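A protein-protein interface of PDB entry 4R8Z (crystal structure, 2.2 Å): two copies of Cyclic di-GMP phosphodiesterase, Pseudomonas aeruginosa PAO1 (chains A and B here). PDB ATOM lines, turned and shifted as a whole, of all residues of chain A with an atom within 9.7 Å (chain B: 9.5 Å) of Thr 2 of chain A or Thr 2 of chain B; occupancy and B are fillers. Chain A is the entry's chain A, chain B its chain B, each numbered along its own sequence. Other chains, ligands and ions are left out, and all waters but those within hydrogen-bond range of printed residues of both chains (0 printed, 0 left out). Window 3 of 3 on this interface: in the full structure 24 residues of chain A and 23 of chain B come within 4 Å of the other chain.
No residue of chain B comes within 4 Å of Arg 1 of chain A. Printed residues of chain B within 4 Å of Thr 2 of chain A: Thr 2 (3.8 Å). Gln 4 of chain A touches none of the printed residues of chain B. Printed residues of chain B within 4 Å of Leu 8 of chain A: Gln 9. Thr 2 of chain B touches one residue of chain A. No residue of chain A comes within 4 Å of Gln 4 of chain B. Printed residues of chain A within 4 Å of Leu 8 of chain B: Gln 9. Of the printed residues of chain A, Gln 9 of chain B touches Leu 8. The nearest residue of chain B that does not touch Thr 2 of chain A is Leu 5 of chain B (4.3 Å). The nearest printed residue of chain B that does not touch Gln 6 of chain A is Leu 8 of chain B (6.2 Å).
Thr 2 of chain A touches its own counterpart, Thr 2 of chain B. Gln 6 of chain A touches Leu 5 of chain B, but with the chains exchanged Leu 5 of chain A does not touch Gln 6 of chain B (4.2 Å). Leu 8 of chain A touches Gln 9 of chain B, and with the chains exchanged Gln 9 of chain A touches Leu 8 of chain B. Positions printed for both chains: 1, 2, 3, 4, 5, 6, 7, 8, 9, 10 and 65. Of the 4 pairs that touch across the chains among the printed residues, 3 have their exchanged pair printed and touching as well.
OE1 of Gln 6 of chain B lies close to OE1 of Gln 9 of chain B (3.1 Å). The side-chain amide oxygen (OE1) of Gln 6 of chain A sits close to the side-chain carboxylate (OD1) of Asp 10 of chain A. The side-chain amide oxygen of Gln 6 of chain A is in hydrogen-bond range of the side-chain amino group of Lys 65 of chain A (2.9 Å).
Among the printed residues, merely in contact across the chains: Thr 2 of chain A with Thr 2 of chain B (3.8 Å), Gln 6 of chain A with Leu 5 of chain B (3.9 Å), Leu 8 of chain A with Gln 9 of chain B (3.5 Å) and Gln 9 of chain A with Leu 8 of chain B (3.2 Å).
Hydrophobic or aromatic side chains of chain B within 4 Å of the printed part of chain A: Leu 5 and Leu 8. Of the 11 printed residues of chain A, 4 touch a printed residue of chain B. Printed residues of chain A that touch a printed residue of chain B: Thr 2, Gln 6, Leu 8 and Gln 9. Hydrophobic or aromatic side chains of chain A within 4 Å of the printed part of chain B: Leu 8. Among the printed residues, 4 pairs touch across the chains.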
ATOM      1  N   ARG A   1       1.259 -25.188 -27.619  1.00  0.00           N
ATOM      2  CA  ARG A   1       1.906 -24.677 -26.416  1.00  0.00           C
ATOM      3  C   ARG A   1       1.558 -23.211 -26.183  1.00  0.00           C
ATOM      4  O   ARG A   1       0.794 -22.881 -25.276  1.00  0.00           O
ATOM      5  CB  ARG A   1       3.424 -24.848 -26.512  1.00  0.00           C
ATOM      6  N   THR A   2       2.123 -22.335 -27.008  1.00  0.00           N
ATOM      7  CA  THR A   2       1.866 -20.860 -26.889  1.00  0.00           C
ATOM      8  C   THR A   2       1.025 -20.347 -28.073  1.00  0.00           C
ATOM      9  O   THR A   2       1.125 -19.211 -28.517  1.00  0.00           O
ATOM     10  CB  THR A   2       3.184 -20.044 -26.962  1.00  0.00           C
ATOM     11  OG1 THR A   2       3.791 -20.199 -28.266  1.00  0.00           O
ATOM     12  CG2 THR A   2       4.166 -20.475 -25.876  1.00  0.00           C
ATOM     13  N   ARG A   3       0.209 -21.235 -28.594  1.00  0.00           N
ATOM     14  CA  ARG A   3      -0.701 -20.899 -29.655  1.00  0.00           C
ATOM     15  C   ARG A   3      -1.660 -19.765 -29.286  1.00  0.00           C
ATOM     16  O   ARG A   3      -1.971 -18.948 -30.136  1.00  0.00           O
ATOM     17  CB  ARG A   3      -1.470 -22.159 -30.089  1.00  0.00           C
ATOM     18  CG  ARG A   3      -0.943 -22.840 -31.358  1.00  0.00           C
ATOM     19  CD  ARG A   3      -1.289 -24.342 -31.428  1.00  0.00           C
ATOM     20  NE  ARG A   3      -2.635 -24.667 -30.904  1.00  0.00           N
ATOM     21  CZ  ARG A   3      -3.014 -25.855 -30.398  1.00  0.00           C
ATOM     22  NH1 ARG A   3      -2.163 -26.892 -30.340  1.00  0.00           N
ATOM     23  NH2 ARG A   3      -4.267 -26.024 -29.962  1.00  0.00           N
ATOM     24  N   GLN A   4      -2.111 -19.707 -28.032  1.00  0.00           N
ATOM     25  CA  GLN A   4      -3.118 -18.730 -27.603  1.00  0.00           C
ATOM     26  C   GLN A   4      -2.693 -17.321 -28.035  1.00  0.00           C
ATOM     27  O   GLN A   4      -3.412 -16.661 -28.755  1.00  0.00           O
ATOM     28  CB  GLN A   4      -3.356 -18.785 -26.078  1.00  0.00           C
ATOM     29  N   LEU A   5      -1.485 -16.907 -27.675  1.00  0.00           N
ATOM     30  CA  LEU A   5      -0.993 -15.615 -28.113  1.00  0.00           C
ATOM     31  C   LEU A   5      -0.770 -15.476 -29.627  1.00  0.00           C
ATOM     32  O   LEU A   5      -0.889 -14.383 -30.140  1.00  0.00           O
ATOM     33  CB  LEU A   5       0.291 -15.224 -27.390  1.00  0.00           C
ATOM     34  CG  LEU A   5       0.114 -14.972 -25.904  1.00  0.00           C
ATOM     35  CD1 LEU A   5       1.444 -14.498 -25.320  1.00  0.00           C
ATOM     36  CD2 LEU A   5      -0.991 -13.966 -25.578  1.00  0.00           C
ATOM     37  N   GLN A   6      -0.395 -16.546 -30.324  1.00  0.00           N
ATOM     38  CA  GLN A   6      -0.063 -16.443 -31.733  1.00  0.00           C
ATOM     39  C   GLN A   6      -1.398 -16.275 -32.490  1.00  0.00           C
ATOM     40  O   GLN A   6      -1.491 -15.544 -33.450  1.00  0.00           O
ATOM     41  CB  GLN A   6       0.712 -17.700 -32.235  1.00  0.00           C
ATOM     42  CG  GLN A   6       1.088 -17.675 -33.717  1.00  0.00           C
ATOM     43  CD  GLN A   6       1.972 -16.472 -34.064  1.00  0.00           C
ATOM     44  OE1 GLN A   6       1.610 -15.598 -34.900  1.00  0.00           O
ATOM     45  NE2 GLN A   6       3.144 -16.419 -33.433  1.00  0.00           N
ATOM     46  N   GLN A   7      -2.419 -16.986 -32.053  1.00  0.00           N
ATOM     47  CA  GLN A   7      -3.707 -16.840 -32.635  1.00  0.00           C
ATOM     48  C   GLN A   7      -4.325 -15.453 -32.351  1.00  0.00           C
ATOM     49  O   GLN A   7      -4.990 -14.872 -33.221  1.00  0.00           O
ATOM     50  CB  GLN A   7      -4.630 -17.918 -32.110  1.00  0.00           C
ATOM     51  CG  GLN A   7      -4.449 -19.233 -32.833  1.00  0.00           C
ATOM     52  CD  GLN A   7      -5.086 -20.397 -32.066  1.00  0.00           C
ATOM     53  OE1 GLN A   7      -6.302 -20.419 -31.815  1.00  0.00           O
ATOM     54  NE2 GLN A   7      -4.274 -21.377 -31.713  1.00  0.00           N
ATOM     55  N   LEU A   8      -4.115 -14.945 -31.146  1.00  0.00           N
ATOM     56  CA  LEU A   8      -4.598 -13.637 -30.825  1.00  0.00           C
ATOM     57  C   LEU A   8      -3.914 -12.595 -31.720  1.00  0.00           C
ATOM     58  O   LEU A   8      -4.594 -11.809 -32.348  1.00  0.00           O
ATOM     59  CB  LEU A   8      -4.333 -13.326 -29.359  1.00  0.00           C
ATOM     60  CG  LEU A   8      -4.600 -11.891 -28.854  1.00  0.00           C
ATOM     61  CD1 LEU A   8      -6.060 -11.582 -29.026  1.00  0.00           C
ATOM     62  CD2 LEU A   8      -4.199 -11.777 -27.385  1.00  0.00           C
ATOM     63  N   GLN A   9      -2.596 -12.627 -31.834  1.00  0.00           N
ATOM     64  CA  GLN A   9      -1.891 -11.735 -32.739  1.00  0.00           C
ATOM     65  C   GLN A   9      -2.474 -11.819 -34.163  1.00  0.00           C
ATOM     66  O   GLN A   9      -2.729 -10.799 -34.796  1.00  0.00           O
ATOM     67  CB  GLN A   9      -0.368 -12.009 -32.768  1.00  0.00           C
ATOM     68  CG  GLN A   9       0.419 -11.293 -33.899  1.00  0.00           C
ATOM     69  CD  GLN A   9       1.909 -11.727 -34.146  1.00  0.00           C
ATOM     70  OE1 GLN A   9       2.715 -11.968 -33.182  1.00  0.00           O
ATOM     71  NE2 GLN A   9       2.253 -11.907 -35.429  1.00  0.00           N
ATOM     72  N   ASP A  10      -2.670 -13.017 -34.674  1.00  0.00           N
ATOM     73  CA  ASP A  10      -3.146 -13.121 -36.039  1.00  0.00           C
ATOM     74  C   ASP A  10      -4.495 -12.469 -36.160  1.00  0.00           C
ATOM     75  O   ASP A  10      -4.772 -11.805 -37.133  1.00  0.00           O
ATOM     76  CB  ASP A  10      -3.244 -14.589 -36.498  1.00  0.00           C
ATOM     77  CG  ASP A  10      -1.856 -15.281 -36.626  1.00  0.00           C
ATOM     78  OD1 ASP A  10      -0.799 -14.582 -36.502  1.00  0.00           O
ATOM     79  OD2 ASP A  10      -1.834 -16.537 -36.843  1.00  0.00           O
ATOM     80  N   LYS A  65       2.366 -13.818 -43.420  1.00  0.00           N
ATOM     81  CA  LYS A  65       1.537 -13.056 -42.472  1.00  0.00           C
ATOM     82  C   LYS A  65       1.849 -11.571 -42.488  1.00  0.00           C
ATOM     83  O   LYS A  65       0.942 -10.757 -42.346  1.00  0.00           O
ATOM     84  CB  LYS A  65       1.653 -13.603 -41.070  1.00  0.00           C
ATOM     85  CG  LYS A  65       0.993 -14.971 -40.997  1.00  0.00           C
ATOM     86  CD  LYS A  65       1.687 -15.893 -40.002  1.00  0.00           C
ATOM     87  CE  LYS A  65       1.496 -15.439 -38.563  1.00  0.00           C
ATOM     88  NZ  LYS A  65       1.331 -16.601 -37.637  1.00  0.00           N
ATOM     89  N   ARG B   1      10.322 -16.637 -24.106  1.00  0.00           N
ATOM     90  CA  ARG B   1       9.651 -17.057 -25.389  1.00  0.00           C
ATOM     91  C   ARG B   1       8.302 -16.423 -25.525  1.00  0.00           C
ATOM     92  O   ARG B   1       7.926 -15.905 -26.578  1.00  0.00           O
ATOM     93  CB  ARG B   1       9.464 -18.573 -25.435  1.00  0.00           C
ATOM     94  N   THR B   2       7.560 -16.493 -24.432  1.00  0.00           N
ATOM     95  CA  THR B   2       6.279 -15.834 -24.332  1.00  0.00           C
ATOM     96  C   THR B   2       6.447 -14.314 -24.249  1.00  0.00           C
ATOM     97  O   THR B   2       5.596 -13.568 -24.717  1.00  0.00           O
ATOM     98  CB  THR B   2       5.509 -16.405 -23.122  1.00  0.00           C
ATOM     99  OG1 THR B   2       4.589 -17.391 -23.611  1.00  0.00           O
ATOM    100  CG2 THR B   2       4.759 -15.324 -22.318  1.00  0.00           C
ATOM    101  N   ARG B   3       7.530 -13.851 -23.642  1.00  0.00           N
ATOM    102  CA  ARG B   3       7.857 -12.442 -23.671  1.00  0.00           C
ATOM    103  C   ARG B   3       8.032 -11.952 -25.100  1.00  0.00           C
ATOM    104  O   ARG B   3       7.435 -10.976 -25.478  1.00  0.00           O
ATOM    105  CB  ARG B   3       9.078 -12.145 -22.785  1.00  0.00           C
ATOM    106  CG  ARG B   3       8.703 -11.989 -21.290  1.00  0.00           C
ATOM    107  CD  ARG B   3       7.464 -11.098 -21.021  1.00  0.00           C
ATOM    108  NE  ARG B   3       7.567  -9.731 -21.577  1.00  0.00           N
ATOM    109  CZ  ARG B   3       8.363  -8.773 -21.091  1.00  0.00           C
ATOM    110  NH1 ARG B   3       8.389  -7.571 -21.701  1.00  0.00           N
ATOM    111  NH2 ARG B   3       9.135  -9.013 -20.004  1.00  0.00           N
ATOM    112  N   GLN B   4       8.809 -12.661 -25.906  1.00  0.00           N
ATOM    113  CA  GLN B   4       9.062 -12.253 -27.263  1.00  0.00           C
ATOM    114  C   GLN B   4       7.713 -11.923 -27.908  1.00  0.00           C
ATOM    115  O   GLN B   4       7.555 -10.864 -28.462  1.00  0.00           O
ATOM    116  CB  GLN B   4       9.801 -13.359 -28.048  1.00  0.00           C
ATOM    117  N   LEU B   5       6.733 -12.813 -27.814  1.00  0.00           N
ATOM    118  CA  LEU B   5       5.412 -12.553 -28.411  1.00  0.00           C
ATOM    119  C   LEU B   5       4.620 -11.445 -27.767  1.00  0.00           C
ATOM    120  O   LEU B   5       3.883 -10.759 -28.453  1.00  0.00           O
ATOM    121  CB  LEU B   5       4.549 -13.802 -28.476  1.00  0.00           C
ATOM    122  CG  LEU B   5       5.068 -14.878 -29.432  1.00  0.00           C
ATOM    123  CD1 LEU B   5       4.094 -16.041 -29.458  1.00  0.00           C
ATOM    124  CD2 LEU B   5       5.318 -14.375 -30.850  1.00  0.00           C
ATOM    125  N   GLN B   6       4.806 -11.221 -26.484  1.00  0.00           N
ATOM    126  CA  GLN B   6       4.040 -10.200 -25.811  1.00  0.00           C
ATOM    127  C   GLN B   6       4.629  -8.855 -26.178  1.00  0.00           C
ATOM    128  O   GLN B   6       3.934  -7.879 -26.362  1.00  0.00           O
ATOM    129  CB  GLN B   6       4.069 -10.427 -24.285  1.00  0.00           C
ATOM    130  CG  GLN B   6       3.215  -9.453 -23.479  1.00  0.00           C
ATOM    131  CD  GLN B   6       1.740  -9.522 -23.888  1.00  0.00           C
ATOM    132  OE1 GLN B   6       1.169  -8.559 -24.414  1.00  0.00           O
ATOM    133  NE2 GLN B   6       1.131 -10.686 -23.684  1.00  0.00           N
ATOM    134  N   GLN B   7       5.927  -8.787 -26.287  1.00  0.00           N
ATOM    135  CA  GLN B   7       6.564  -7.551 -26.705  1.00  0.00           C
ATOM    136  C   GLN B   7       6.253  -7.227 -28.166  1.00  0.00           C
ATOM    137  O   GLN B   7       6.010  -6.092 -28.522  1.00  0.00           O
ATOM    138  CB  GLN B   7       8.069  -7.647 -26.556  1.00  0.00           C
ATOM    139  CG  GLN B   7       8.610  -7.479 -25.143  1.00  0.00           C
ATOM    140  CD  GLN B   7      10.093  -7.884 -25.031  1.00  0.00           C
ATOM    141  OE1 GLN B   7      10.966  -7.328 -25.707  1.00  0.00           O
ATOM    142  NE2 GLN B   7      10.368  -8.859 -24.183  1.00  0.00           N
ATOM    143  N   LEU B   8       6.229  -8.229 -29.001  1.00  0.00           N
ATOM    144  CA  LEU B   8       5.836  -8.043 -30.382  1.00  0.00           C
ATOM    145  C   LEU B   8       4.390  -7.498 -30.433  1.00  0.00           C
ATOM    146  O   LEU B   8       4.158  -6.463 -31.043  1.00  0.00           O
ATOM    147  CB  LEU B   8       5.957  -9.353 -31.144  1.00  0.00           C
ATOM    148  CG  LEU B   8       5.461  -9.358 -32.571  1.00  0.00           C
ATOM    149  CD1 LEU B   8       6.240  -8.372 -33.410  1.00  0.00           C
ATOM    150  CD2 LEU B   8       5.637 -10.765 -33.151  1.00  0.00           C
ATOM    151  N   GLN B   9       3.434  -8.142 -29.773  1.00  0.00           N
ATOM    152  CA  GLN B   9       2.048  -7.632 -29.767  1.00  0.00           C
ATOM    153  C   GLN B   9       1.984  -6.165 -29.323  1.00  0.00           C
ATOM    154  O   GLN B   9       1.330  -5.358 -29.975  1.00  0.00           O
ATOM    155  CB  GLN B   9       1.134  -8.507 -28.886  1.00  0.00           C
ATOM    156  CG  GLN B   9      -0.238  -7.897 -28.556  1.00  0.00           C
ATOM    157  CD  GLN B   9      -0.946  -8.609 -27.375  1.00  0.00           C
ATOM    158  OE1 GLN B   9      -1.197  -8.008 -26.300  1.00  0.00           O
ATOM    159  NE2 GLN B   9      -1.229  -9.910 -27.559  1.00  0.00           N
ATOM    160  N   ASP B  10       2.679  -5.810 -28.237  1.00  0.00           N
ATOM    161  CA  ASP B  10       2.647  -4.442 -27.756  1.00  0.00           C
ATOM    162  C   ASP B  10       3.189  -3.509 -28.790  1.00  0.00           C
ATOM    163  O   ASP B  10       2.657  -2.446 -29.000  1.00  0.00           O
ATOM    164  CB  ASP B  10       3.442  -4.259 -26.468  1.00  0.00           C
ATOM    165  CG  ASP B  10       2.823  -5.037 -25.293  1.00  0.00           C
ATOM    166  OD1 ASP B  10       1.737  -5.647 -25.489  1.00  0.00           O
ATOM    167  OD2 ASP B  10       3.430  -5.089 -24.183  1.00  0.00           O
ATOM    168  N   LYS B  65      -3.745  -1.879 -21.854  1.00  0.00           N
ATOM    169  CA  LYS B  65      -3.204  -1.994 -23.246  1.00  0.00           C
ATOM    170  C   LYS B  65      -4.314  -1.860 -24.268  1.00  0.00           C
ATOM    171  O   LYS B  65      -4.116  -1.269 -25.337  1.00  0.00           O
ATOM    172  CB  LYS B  65      -2.441  -3.302 -23.429  1.00  0.00           C
ATOM    173  CG  LYS B  65      -1.155  -3.239 -22.631  1.00  0.00           C
ATOM    174  CD  LYS B  65      -0.739  -4.573 -22.040  1.00  0.00           C
ATOM    175  CE  LYS B  65      -0.311  -5.549 -23.110  1.00  0.00           C
ATOM    176  NZ  LYS B  65       0.829  -6.373 -22.611  1.00  0.00           N
